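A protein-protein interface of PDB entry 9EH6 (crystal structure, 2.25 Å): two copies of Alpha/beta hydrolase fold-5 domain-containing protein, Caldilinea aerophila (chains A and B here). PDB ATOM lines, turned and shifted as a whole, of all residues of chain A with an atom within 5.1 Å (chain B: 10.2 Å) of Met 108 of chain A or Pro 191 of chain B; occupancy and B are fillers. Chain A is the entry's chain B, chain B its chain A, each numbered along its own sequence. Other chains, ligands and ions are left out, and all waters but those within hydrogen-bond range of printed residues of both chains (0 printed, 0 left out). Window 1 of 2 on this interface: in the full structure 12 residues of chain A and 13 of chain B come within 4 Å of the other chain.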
ATOM      1  N   TYR A  43     -22.667   2.416   2.447  1.00  0.00           N
ATOM      2  CA  TYR A  43     -23.189   3.730   2.786  1.00  0.00           C
ATOM      3  C   TYR A  43     -24.561   3.603   3.453  1.00  0.00           C
ATOM      4  O   TYR A  43     -25.495   3.050   2.875  1.00  0.00           O
ATOM      5  CB  TYR A  43     -23.344   4.572   1.519  1.00  0.00           C
ATOM      6  CG  TYR A  43     -22.059   5.107   0.905  1.00  0.00           C
ATOM      7  CD1 TYR A  43     -20.810   4.811   1.452  1.00  0.00           C
ATOM      8  CD2 TYR A  43     -22.092   5.902  -0.235  1.00  0.00           C
ATOM      9  CE1 TYR A  43     -19.640   5.319   0.909  1.00  0.00           C
ATOM     10  CE2 TYR A  43     -20.921   6.389  -0.803  1.00  0.00           C
ATOM     11  CZ  TYR A  43     -19.691   6.103  -0.236  1.00  0.00           C
ATOM     12  OH  TYR A  43     -18.531   6.576  -0.785  1.00  0.00           O
ATOM     13  N   ALA A  81     -19.580  11.685  -0.358  1.00  0.00           N
ATOM     14  CA  ALA A  81     -19.977  10.634  -1.329  1.00  0.00           C
ATOM     15  C   ALA A  81     -18.768   9.825  -1.817  1.00  0.00           C
ATOM     16  O   ALA A  81     -18.948   8.720  -2.333  1.00  0.00           O
ATOM     17  CB  ALA A  81     -20.734  11.251  -2.485  1.00  0.00           C
ATOM     18  N   ARG A  83     -16.089   9.470   0.352  1.00  0.00           N
ATOM     19  CA  ARG A  83     -15.558   9.008   1.618  1.00  0.00           C
ATOM     20  C   ARG A  83     -15.043   7.576   1.443  1.00  0.00           C
ATOM     21  O   ARG A  83     -14.371   7.031   2.307  1.00  0.00           O
ATOM     22  CB  ARG A  83     -16.682   9.156   2.647  1.00  0.00           C
ATOM     23  CG  ARG A  83     -17.849   8.203   2.451  1.00  0.00           C
ATOM     24  CD  ARG A  83     -19.203   8.882   2.337  1.00  0.00           C
ATOM     25  NE  ARG A  83     -20.234   8.127   3.024  1.00  0.00           N
ATOM     26  CZ  ARG A  83     -21.552   8.267   2.864  1.00  0.00           C
ATOM     27  NH1 ARG A  83     -22.367   7.680   3.722  1.00  0.00           N
ATOM     28  NH2 ARG A  83     -22.052   9.002   1.884  1.00  0.00           N
ATOM     29  N   LEU A 104     -30.985   6.379   0.117  1.00  0.00           N
ATOM     30  CA  LEU A 104     -30.123   7.498  -0.283  1.00  0.00           C
ATOM     31  C   LEU A 104     -28.631   7.135  -0.303  1.00  0.00           C
ATOM     32  O   LEU A 104     -27.865   7.671  -1.098  1.00  0.00           O
ATOM     33  CB  LEU A 104     -30.363   8.651   0.697  1.00  0.00           C
ATOM     34  CG  LEU A 104     -30.984   9.938   0.142  1.00  0.00           C
ATOM     35  CD1 LEU A 104     -32.324   9.698  -0.520  1.00  0.00           C
ATOM     36  CD2 LEU A 104     -31.094  10.995   1.248  1.00  0.00           C
ATOM     37  N   GLY A 105     -28.202   6.246   0.598  1.00  0.00           N
ATOM     38  CA  GLY A 105     -26.829   5.764   0.628  1.00  0.00           C
ATOM     39  C   GLY A 105     -26.456   5.030  -0.662  1.00  0.00           C
ATOM     40  O   GLY A 105     -25.353   5.197  -1.179  1.00  0.00           O
ATOM     41  N   GLY A 106     -27.392   4.210  -1.165  1.00  0.00           N
ATOM     42  CA  GLY A 106     -27.184   3.520  -2.423  1.00  0.00           C
ATOM     43  C   GLY A 106     -27.042   4.489  -3.597  1.00  0.00           C
ATOM     44  O   GLY A 106     -26.255   4.233  -4.505  1.00  0.00           O
ATOM     45  N   ALA A 107     -27.818   5.579  -3.589  1.00  0.00           N
ATOM     46  CA  ALA A 107     -27.734   6.594  -4.627  1.00  0.00           C
ATOM     47  C   ALA A 107     -26.328   7.176  -4.640  1.00  0.00           C
ATOM     48  O   ALA A 107     -25.710   7.290  -5.711  1.00  0.00           O
ATOM     49  CB  ALA A 107     -28.775   7.675  -4.412  1.00  0.00           C
ATOM     50  N   MET A 108     -25.850   7.516  -3.434  1.00  0.00           N
ATOM     51  CA  MET A 108     -24.529   8.093  -3.210  1.00  0.00           C
ATOM     52  C   MET A 108     -23.441   7.110  -3.676  1.00  0.00           C
ATOM     53  O   MET A 108     -22.423   7.502  -4.258  1.00  0.00           O
ATOM     54  CB  MET A 108     -24.334   8.364  -1.711  1.00  0.00           C
ATOM     55  CG  MET A 108     -25.024   9.604  -1.151  1.00  0.00           C
ATOM     56  SD  MET A 108     -23.889  11.014  -1.181  1.00  0.00           S
ATOM     57  CE  MET A 108     -24.138  11.636  -2.852  1.00  0.00           C
ATOM     58  N   ALA A 109     -23.662   5.808  -3.430  1.00  0.00           N
ATOM     59  CA  ALA A 109     -22.698   4.802  -3.848  1.00  0.00           C
ATOM     60  C   ALA A 109     -22.636   4.729  -5.381  1.00  0.00           C
ATOM     61  O   ALA A 109     -21.544   4.721  -5.962  1.00  0.00           O
ATOM     62  CB  ALA A 109     -23.020   3.481  -3.205  1.00  0.00           C
ATOM     63  N   ALA A 110     -23.822   4.720  -6.017  1.00  0.00           N
ATOM     64  CA  ALA A 110     -23.933   4.768  -7.465  1.00  0.00           C
ATOM     65  C   ALA A 110     -23.178   5.986  -7.996  1.00  0.00           C
ATOM     66  O   ALA A 110     -22.509   5.913  -9.019  1.00  0.00           O
ATOM     67  CB  ALA A 110     -25.390   4.816  -7.883  1.00  0.00           C
ATOM     68  N   ASN A 111     -23.252   7.084  -7.248  1.00  0.00           N
ATOM     69  CA  ASN A 111     -22.680   8.347  -7.671  1.00  0.00           C
ATOM     70  C   ASN A 111     -21.158   8.237  -7.699  1.00  0.00           C
ATOM     71  O   ASN A 111     -20.551   8.588  -8.710  1.00  0.00           O
ATOM     72  CB  ASN A 111     -23.196   9.522  -6.837  1.00  0.00           C
ATOM     73  CG  ASN A 111     -22.631  10.848  -7.303  1.00  0.00           C
ATOM     74  OD1 ASN A 111     -21.754  11.421  -6.654  1.00  0.00           O
ATOM     75  ND2 ASN A 111     -23.106  11.329  -8.442  1.00  0.00           N
ATOM     76  N   PHE A 112     -20.576   7.739  -6.594  1.00  0.00           N
ATOM     77  CA  PHE A 112     -19.144   7.464  -6.510  1.00  0.00           C
ATOM     78  C   PHE A 112     -18.698   6.594  -7.693  1.00  0.00           C
ATOM     79  O   PHE A 112     -17.713   6.920  -8.346  1.00  0.00           O
ATOM     80  CB  PHE A 112     -18.754   6.793  -5.184  1.00  0.00           C
ATOM     81  CG  PHE A 112     -17.272   6.540  -5.073  1.00  0.00           C
ATOM     82  CD1 PHE A 112     -16.397   7.568  -4.747  1.00  0.00           C
ATOM     83  CD2 PHE A 112     -16.737   5.299  -5.390  1.00  0.00           C
ATOM     84  CE1 PHE A 112     -15.027   7.359  -4.727  1.00  0.00           C
ATOM     85  CE2 PHE A 112     -15.369   5.087  -5.364  1.00  0.00           C
ATOM     86  CZ  PHE A 112     -14.515   6.118  -5.041  1.00  0.00           C
ATOM     87  N   ALA A 131     -29.316   8.079  -9.516  1.00  0.00           N
ATOM     88  CA  ALA A 131     -29.894   9.279 -10.095  1.00  0.00           C
ATOM     89  C   ALA A 131     -29.783   9.210 -11.617  1.00  0.00           C
ATOM     90  O   ALA A 131     -28.919   8.507 -12.167  1.00  0.00           O
ATOM     91  CB  ALA A 131     -29.168  10.497  -9.577  1.00  0.00           C
ATOM     92  N   SER A 133     -28.571  11.441 -13.551  1.00  0.00           N
ATOM     93  CA  SER A 133     -27.262  11.855 -14.023  1.00  0.00           C
ATOM     94  C   SER A 133     -26.189  10.793 -13.777  1.00  0.00           C
ATOM     95  O   SER A 133     -25.100  10.937 -14.320  1.00  0.00           O
ATOM     96  CB  SER A 133     -26.852  13.173 -13.400  1.00  0.00           C
ATOM     97  OG  SER A 133     -26.688  13.040 -11.987  1.00  0.00           O
ATOM     98  N   ASP A 134     -26.493   9.739 -12.987  1.00  0.00           N
ATOM     99  CA  ASP A 134     -25.488   8.740 -12.652  1.00  0.00           C
ATOM    100  C   ASP A 134     -25.675   7.418 -13.402  1.00  0.00           C
ATOM    101  O   ASP A 134     -25.285   6.369 -12.888  1.00  0.00           O
ATOM    102  CB  ASP A 134     -25.437   8.480 -11.142  1.00  0.00           C
ATOM    103  CG  ASP A 134     -24.740   9.591 -10.369  1.00  0.00           C
ATOM    104  OD1 ASP A 134     -23.734  10.123 -10.871  1.00  0.00           O
ATOM    105  OD2 ASP A 134     -25.197   9.902  -9.248  1.00  0.00           O
ATOM    106  N   MET B   2     -19.591  17.578 -15.262  1.00  0.00           N
ATOM    107  CA  MET B   2     -20.409  18.518 -14.451  1.00  0.00           C
ATOM    108  C   MET B   2     -21.895  18.259 -14.749  1.00  0.00           C
ATOM    109  O   MET B   2     -22.249  17.858 -15.859  1.00  0.00           O
ATOM    110  CB  MET B   2     -20.012  19.971 -14.772  1.00  0.00           C
ATOM    111  CG  MET B   2     -18.664  20.420 -14.182  1.00  0.00           C
ATOM    112  N   LEU B   3     -22.763  18.446 -13.735  1.00  0.00           N
ATOM    113  CA  LEU B   3     -24.216  18.473 -13.885  1.00  0.00           C
ATOM    114  C   LEU B   3     -24.614  19.729 -14.664  1.00  0.00           C
ATOM    115  O   LEU B   3     -24.251  20.841 -14.270  1.00  0.00           O
ATOM    116  CB  LEU B   3     -24.859  18.480 -12.492  1.00  0.00           C
ATOM    117  CG  LEU B   3     -24.408  17.343 -11.578  1.00  0.00           C
ATOM    118  CD1 LEU B   3     -25.032  17.467 -10.190  1.00  0.00           C
ATOM    119  CD2 LEU B   3     -24.737  15.986 -12.203  1.00  0.00           C
ATOM    120  N   GLN B   4     -25.393  19.527 -15.739  1.00  0.00           N
ATOM    121  CA  GLN B   4     -25.550  20.498 -16.813  1.00  0.00           C
ATOM    122  C   GLN B   4     -26.688  21.459 -16.493  1.00  0.00           C
ATOM    123  O   GLN B   4     -27.640  21.062 -15.820  1.00  0.00           O
ATOM    124  CB  GLN B   4     -25.860  19.764 -18.123  1.00  0.00           C
ATOM    125  CG  GLN B   4     -24.649  19.079 -18.748  1.00  0.00           C
ATOM    126  CD  GLN B   4     -23.601  20.115 -19.062  1.00  0.00           C
ATOM    127  OE1 GLN B   4     -23.848  21.026 -19.845  1.00  0.00           O
ATOM    128  NE2 GLN B   4     -22.443  20.007 -18.432  1.00  0.00           N
ATOM    129  N   GLY B  46     -20.198  21.870  -5.938  1.00  0.00           N
ATOM    130  CA  GLY B  46     -19.255  20.938  -6.537  1.00  0.00           C
ATOM    131  C   GLY B  46     -19.916  20.216  -7.707  1.00  0.00           C
ATOM    132  O   GLY B  46     -21.062  19.783  -7.590  1.00  0.00           O
ATOM    133  N   ARG B  47     -19.211  20.191  -8.843  1.00  0.00           N
ATOM    134  CA  ARG B  47     -19.595  19.491 -10.060  1.00  0.00           C
ATOM    135  C   ARG B  47     -20.811  20.103 -10.757  1.00  0.00           C
ATOM    136  O   ARG B  47     -21.368  19.459 -11.641  1.00  0.00           O
ATOM    137  CB  ARG B  47     -19.856  18.006  -9.791  1.00  0.00           C
ATOM    138  CG  ARG B  47     -18.627  17.245  -9.312  1.00  0.00           C
ATOM    139  CD  ARG B  47     -18.942  15.772  -9.135  1.00  0.00           C
ATOM    140  NE  ARG B  47     -17.762  15.043  -8.681  1.00  0.00           N
ATOM    141  CZ  ARG B  47     -16.832  14.497  -9.466  1.00  0.00           C
ATOM    142  NH1 ARG B  47     -16.950  14.552 -10.783  1.00  0.00           N
ATOM    143  NH2 ARG B  47     -15.804  13.867  -8.920  1.00  0.00           N
ATOM    144  N   VAL B  48     -21.216  21.325 -10.385  1.00  0.00           N
ATOM    145  CA  VAL B  48     -22.358  21.952 -11.034  1.00  0.00           C
ATOM    146  C   VAL B  48     -21.870  22.975 -12.061  1.00  0.00           C
ATOM    147  O   VAL B  48     -21.045  23.817 -11.747  1.00  0.00           O
ATOM    148  CB  VAL B  48     -23.352  22.578 -10.029  1.00  0.00           C
ATOM    149  CG1 VAL B  48     -24.496  23.283 -10.757  1.00  0.00           C
ATOM    150  CG2 VAL B  48     -23.898  21.567  -9.026  1.00  0.00           C
ATOM    151  N   HIS B 102     -23.202  27.793  -2.962  1.00  0.00           N
ATOM    152  CA  HIS B 102     -24.055  26.630  -2.764  1.00  0.00           C
ATOM    153  C   HIS B 102     -23.193  25.435  -2.362  1.00  0.00           C
ATOM    154  O   HIS B 102     -22.199  25.124  -3.018  1.00  0.00           O
ATOM    155  CB  HIS B 102     -24.782  26.323  -4.072  1.00  0.00           C
ATOM    156  CG  HIS B 102     -25.703  25.167  -4.006  1.00  0.00           C
ATOM    157  ND1 HIS B 102     -25.834  24.325  -5.085  1.00  0.00           N
ATOM    158  CD2 HIS B 102     -26.578  24.733  -3.073  1.00  0.00           C
ATOM    159  CE1 HIS B 102     -26.771  23.426  -4.804  1.00  0.00           C
ATOM    160  NE2 HIS B 102     -27.206  23.640  -3.588  1.00  0.00           N
ATOM    161  N   SER B 103     -23.559  24.808  -1.245  1.00  0.00           N
ATOM    162  CA  SER B 103     -22.994  23.523  -0.881  1.00  0.00           C
ATOM    163  C   SER B 103     -21.489  23.693  -0.676  1.00  0.00           C
ATOM    164  O   SER B 103     -21.089  24.572   0.078  1.00  0.00           O
ATOM    165  CB  SER B 103     -23.359  22.488  -1.919  1.00  0.00           C
ATOM    166  OG  SER B 103     -23.278  21.200  -1.351  1.00  0.00           O
ATOM    167  N   ASP B 152     -33.645  18.910   2.231  1.00  0.00           N
ATOM    168  CA  ASP B 152     -32.322  18.724   1.656  1.00  0.00           C
ATOM    169  C   ASP B 152     -31.708  17.410   2.160  1.00  0.00           C
ATOM    170  O   ASP B 152     -31.574  17.203   3.361  1.00  0.00           O
ATOM    171  CB  ASP B 152     -31.463  19.977   1.873  1.00  0.00           C
ATOM    172  CG  ASP B 152     -30.047  19.892   1.322  1.00  0.00           C
ATOM    173  OD1 ASP B 152     -29.563  18.760   1.136  1.00  0.00           O
ATOM    174  OD2 ASP B 152     -29.440  20.972   1.062  1.00  0.00           O
ATOM    175  N   GLY B 153     -31.294  16.534   1.231  1.00  0.00           N
ATOM    176  CA  GLY B 153     -30.810  15.220   1.619  1.00  0.00           C
ATOM    177  C   GLY B 153     -29.303  15.187   1.876  1.00  0.00           C
ATOM    178  O   GLY B 153     -28.812  14.219   2.454  1.00  0.00           O
ATOM    179  N   LEU B 154     -28.564  16.224   1.442  1.00  0.00           N
ATOM    180  CA  LEU B 154     -27.106  16.223   1.586  1.00  0.00           C
ATOM    181  C   LEU B 154     -26.704  17.061   2.792  1.00  0.00           C
ATOM    182  O   LEU B 154     -26.026  16.578   3.684  1.00  0.00           O
ATOM    183  CB  LEU B 154     -26.438  16.783   0.331  1.00  0.00           C
ATOM    184  CG  LEU B 154     -26.195  15.787  -0.796  1.00  0.00           C
ATOM    185  CD1 LEU B 154     -27.514  15.338  -1.397  1.00  0.00           C
ATOM    186  CD2 LEU B 154     -25.324  16.422  -1.874  1.00  0.00           C
ATOM    187  N   ALA B 155     -27.136  18.323   2.812  1.00  0.00           N
ATOM    188  CA  ALA B 155     -26.935  19.166   3.970  1.00  0.00           C
ATOM    189  C   ALA B 155     -28.280  19.273   4.684  1.00  0.00           C
ATOM    190  O   ALA B 155     -29.081  20.145   4.335  1.00  0.00           O
ATOM    191  CB  ALA B 155     -26.446  20.505   3.484  1.00  0.00           C
ATOM    192  N   ASN B 180     -35.238  21.470  -1.281  1.00  0.00           N
ATOM    193  CA  ASN B 180     -34.153  20.501  -1.249  1.00  0.00           C
ATOM    194  C   ASN B 180     -32.840  21.142  -1.705  1.00  0.00           C
ATOM    195  O   ASN B 180     -32.732  22.362  -1.820  1.00  0.00           O
ATOM    196  CB  ASN B 180     -34.459  19.258  -2.089  1.00  0.00           C
ATOM    197  CG  ASN B 180     -34.571  19.576  -3.567  1.00  0.00           C
ATOM    198  OD1 ASN B 180     -34.339  20.710  -3.972  1.00  0.00           O
ATOM    199  ND2 ASN B 180     -34.928  18.585  -4.373  1.00  0.00           N
ATOM    200  N   HIS B 181     -31.833  20.290  -1.930  1.00  0.00           N
ATOM    201  CA  HIS B 181     -30.479  20.718  -2.216  1.00  0.00           C
ATOM    202  C   HIS B 181     -30.379  21.253  -3.639  1.00  0.00           C
ATOM    203  O   HIS B 181     -29.721  22.271  -3.865  1.00  0.00           O
ATOM    204  CB  HIS B 181     -29.509  19.538  -2.193  1.00  0.00           C
ATOM    205  CG  HIS B 181     -28.083  19.943  -2.059  1.00  0.00           C
ATOM    206  ND1 HIS B 181     -27.611  20.412  -0.850  1.00  0.00           N
ATOM    207  CD2 HIS B 181     -27.015  19.888  -2.890  1.00  0.00           C
ATOM    208  CE1 HIS B 181     -26.303  20.643  -0.943  1.00  0.00           C
ATOM    209  NE2 HIS B 181     -25.921  20.337  -2.174  1.00  0.00           N
ATOM    210  N   ALA B 182     -31.024  20.539  -4.570  1.00  0.00           N
ATOM    211  CA  ALA B 182     -30.862  20.738  -6.004  1.00  0.00           C
ATOM    212  C   ALA B 182     -31.479  22.052  -6.484  1.00  0.00           C
ATOM    213  O   ALA B 182     -31.018  22.613  -7.475  1.00  0.00           O
ATOM    214  CB  ALA B 182     -31.442  19.568  -6.758  1.00  0.00           C
ATOM    215  N   GLN B 183     -32.543  22.513  -5.801  1.00  0.00           N
ATOM    216  CA  GLN B 183     -33.348  23.624  -6.289  1.00  0.00           C
ATOM    217  C   GLN B 183     -32.697  24.957  -5.890  1.00  0.00           C
ATOM    218  O   GLN B 183     -33.312  26.008  -6.078  1.00  0.00           O
ATOM    219  CB  GLN B 183     -34.818  23.440  -5.877  1.00  0.00           C
ATOM    220  CG  GLN B 183     -35.542  22.334  -6.639  1.00  0.00           C
ATOM    221  CD  GLN B 183     -37.052  22.245  -6.485  1.00  0.00           C
ATOM    222  OE1 GLN B 183     -37.696  21.515  -7.223  1.00  0.00           O
ATOM    223  NE2 GLN B 183     -37.656  23.006  -5.578  1.00  0.00           N
ATOM    224  N   TYR B 187     -30.244  22.755 -12.456  1.00  0.00           N
ATOM    225  CA  TYR B 187     -29.437  21.675 -13.013  1.00  0.00           C
ATOM    226  C   TYR B 187     -30.259  20.384 -12.934  1.00  0.00           C
ATOM    227  O   TYR B 187     -31.487  20.422 -12.888  1.00  0.00           O
ATOM    228  CB  TYR B 187     -27.998  21.751 -12.471  1.00  0.00           C
ATOM    229  CG  TYR B 187     -27.843  21.503 -10.975  1.00  0.00           C
ATOM    230  CD1 TYR B 187     -27.714  20.205 -10.468  1.00  0.00           C
ATOM    231  CD2 TYR B 187     -27.850  22.569 -10.062  1.00  0.00           C
ATOM    232  CE1 TYR B 187     -27.590  19.971  -9.103  1.00  0.00           C
ATOM    233  CE2 TYR B 187     -27.730  22.343  -8.697  1.00  0.00           C
ATOM    234  CZ  TYR B 187     -27.588  21.043  -8.219  1.00  0.00           C
ATOM    235  OH  TYR B 187     -27.442  20.821  -6.878  1.00  0.00           O
ATOM    236  N   GLY B 188     -29.632  19.215 -12.909  1.00  0.00           N
ATOM    237  CA  GLY B 188     -30.514  18.049 -12.788  1.00  0.00           C
ATOM    238  C   GLY B 188     -31.304  17.953 -11.463  1.00  0.00           C
ATOM    239  O   GLY B 188     -31.414  18.900 -10.684  1.00  0.00           O
ATOM    240  N   GLU B 189     -31.823  16.754 -11.193  1.00  0.00           N
ATOM    241  CA  GLU B 189     -32.005  16.272  -9.831  1.00  0.00           C
ATOM    242  C   GLU B 189     -30.598  16.135  -9.246  1.00  0.00           C
ATOM    243  O   GLU B 189     -29.626  16.094  -9.996  1.00  0.00           O
ATOM    244  CB  GLU B 189     -32.892  15.011  -9.833  1.00  0.00           C
ATOM    245  CG  GLU B 189     -34.341  15.294 -10.308  1.00  0.00           C
ATOM    246  CD  GLU B 189     -35.291  14.185 -10.791  1.00  0.00           C
ATOM    247  OE1 GLU B 189     -36.376  14.528 -11.379  1.00  0.00           O
ATOM    248  OE2 GLU B 189     -34.983  12.971 -10.584  1.00  0.00           O
ATOM    249  N   GLN B 190     -30.467  16.168  -7.918  1.00  0.00           N
ATOM    250  CA  GLN B 190     -29.159  16.066  -7.300  1.00  0.00           C
ATOM    251  C   GLN B 190     -28.992  14.652  -6.754  1.00  0.00           C
ATOM    252  O   GLN B 190     -29.815  14.206  -5.948  1.00  0.00           O
ATOM    253  CB  GLN B 190     -29.014  17.094  -6.170  1.00  0.00           C
ATOM    254  CG  GLN B 190     -27.826  16.844  -5.231  1.00  0.00           C
ATOM    255  CD  GLN B 190     -26.539  17.502  -5.671  1.00  0.00           C
ATOM    256  OE1 GLN B 190     -26.508  18.678  -6.018  1.00  0.00           O
ATOM    257  NE2 GLN B 190     -25.447  16.757  -5.655  1.00  0.00           N
ATOM    258  N   PRO B 191     -27.922  13.924  -7.171  1.00  0.00           N
ATOM    259  CA  PRO B 191     -27.573  12.630  -6.581  1.00  0.00           C
ATOM    260  C   PRO B 191     -27.480  12.741  -5.063  1.00  0.00           C
ATOM    261  O   PRO B 191     -26.776  13.617  -4.560  1.00  0.00           O
ATOM    262  CB  PRO B 191     -26.170  12.342  -7.156  1.00  0.00           C
ATOM    263  CG  PRO B 191     -26.143  13.080  -8.490  1.00  0.00           C
ATOM    264  CD  PRO B 191     -26.985  14.319  -8.248  1.00  0.00           C
ATOM    265  N   GLY B 192     -28.218  11.873  -4.359  1.00  0.00           N
ATOM    266  CA  GLY B 192     -28.238  11.810  -2.903  1.00  0.00           C
ATOM    267  C   GLY B 192     -29.320  12.660  -2.224  1.00  0.00           C
ATOM    268  O   GLY B 192     -29.461  12.607  -1.001  1.00  0.00           O
ATOM    269  N   ASP B 193     -30.088  13.444  -3.003  1.00  0.00           N
ATOM    270  CA  ASP B 193     -31.015  14.421  -2.437  1.00  0.00           C
ATOM    271  C   ASP B 193     -32.397  13.777  -2.311  1.00  0.00           C
ATOM    272  O   ASP B 193     -32.597  12.647  -2.763  1.00  0.00           O
ATOM    273  CB  ASP B 193     -31.062  15.653  -3.341  1.00  0.00           C
ATOM    274  CG  ASP B 193     -31.733  16.912  -2.806  1.00  0.00           C
ATOM    275  OD1 ASP B 193     -31.956  17.022  -1.584  1.00  0.00           O
ATOM    276  OD2 ASP B 193     -32.007  17.798  -3.646  1.00  0.00           O
ATOM    277  N   ASN B 194     -33.340  14.486  -1.675  1.00  0.00           N
ATOM    278  CA  ASN B 194     -34.733  14.063  -1.664  1.00  0.00           C
ATOM    279  C   ASN B 194     -35.491  14.930  -2.657  1.00  0.00           C
ATOM    280  O   ASN B 194     -35.004  15.985  -3.029  1.00  0.00           O
ATOM    281  CB  ASN B 194     -35.389  14.253  -0.291  1.00  0.00           C
ATOM    282  CG  ASN B 194     -34.752  13.425   0.802  1.00  0.00           C
ATOM    283  OD1 ASN B 194     -34.775  12.198   0.750  1.00  0.00           O
ATOM    284  ND2 ASN B 194     -34.202  14.074   1.814  1.00  0.00           N
ATOM    285  N   PRO B 195     -36.711  14.536  -3.082  1.00  0.00           N
ATOM    286  CA  PRO B 195     -37.594  15.438  -3.827  1.00  0.00           C
ATOM    287  C   PRO B 195     -38.122  16.612  -2.991  1.00  0.00           C
ATOM    288  O   PRO B 195     -38.414  16.462  -1.815  1.00  0.00           O
ATOM    289  CB  PRO B 195     -38.775  14.533  -4.226  1.00  0.00           C
ATOM    290  CG  PRO B 195     -38.306  13.103  -3.981  1.00  0.00           C
ATOM    291  CD  PRO B 195     -37.296  13.199  -2.857  1.00  0.00           C
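The backbone NH (N) of Leu 3 of chain B sits at hydrogen-bond distance from the backbone carbonyl oxygen (O) of Arg 47 of chain B, 2.7 Å away.
The side-chain carboxylate of Asp 193 of chain B sits at hydrogen-bond distance from the backbone NH of Gly 153 of chain B (2.9 Å).
ND2 of Asn 180 of chain B lies within hydrogen-bond range of OD2 of Asp 193 of chain B, 3.1 Å away.
The backbone NH (N) of His 181 of chain B sits at hydrogen-bond distance from the side-chain carboxylate (OD2) of Asp 193 of chain B (3.0 Å).
N of Ala 182 of chain B sits at hydrogen-bond distance from OD2 of Asp 193 of chain B (3.1 Å).
The side-chain amide nitrogen of Asn 111 of chain A is in hydrogen-bond range of the side-chain carboxylate of Asp 134 of chain A (2.7 Å).
Leu 104 of chain A touches Gly 192 of chain B (CD2 to O, 3.2 Å).
Asp 193 of chain B touches Leu 104 of chain A.
Asn 194 of chain B touches Leu 104 of chain A (OD1 to CD1, 3.7 Å).
Pro 191 of chain B touches Met 108 of chain A.
CB of Pro 191 of chain B touches ND2 of Asn 111 of chain A, 3.5 Å away.
Ser 133 of chain A touches Leu 3 of chain B (OG to CD2, 3.5 Å).
Pro 191 of chain B touches Ser 133 of chain A.
Asp 134 of chain A touches Pro 191 of chain B.
No residue of chain B comes within 4 Å of Ala 81 of chain A.
Of the printed residues of chain B, Leu 104 of chain A touches Gly 192 (3.2 Å), Asp 193 (3.7 Å) and Asn 194 (3.7 Å).
No residue of chain B comes within 4 Å of Gly 105 of chain A.
No residue of chain B comes within 4 Å of Ala 107 of chain A.
Of chain B, only Pro 191 (3.7 Å) comes within 4 Å of Met 108 of chain A.
Ala 109 of chain A touches none of the printed residues of chain B.
Of chain B, only Pro 191 comes within 4 Å of Asn 111 of chain A.
Of the printed residues of chain B, Asp 134 of chain A touches Pro 191 (3.4 Å).
Printed residues of chain A within 4 Å of Leu 3 of chain B: Ser 133 (3.5 Å).
Printed residues of chain A within 4 Å of Asp 193 of chain B: Leu 104 (3.7 Å).
Of the printed residues of chain A, Asn 194 of chain B touches Leu 104 (3.7 Å).
The nearest residue of chain B that does not touch Met 108 of chain A is Gly 192 of chain B (4.1 Å).
The nearest printed residue of chain A that does not touch Pro 191 of chain B is Ala 131 of chain A (4.01 Å).
Printed residues of chain B that touch a printed residue of chain A: Leu 3, Pro 191, Gly 192, Asp 193 and Asn 194.
Hydrophobic or aromatic side chains of chain B that line the printed part of chain A: Leu 3 and Pro 191.
Along chain B the printed residues that touch a printed residue of chain A span positions 3 to 194.
Of the 15 printed residues of chain A, 5 touch a printed residue of chain B.
No position is printed for both chains.
Of the 8 pairs that touch across the chains among the printed residues, none has its exchanged pair printed and touching as well.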
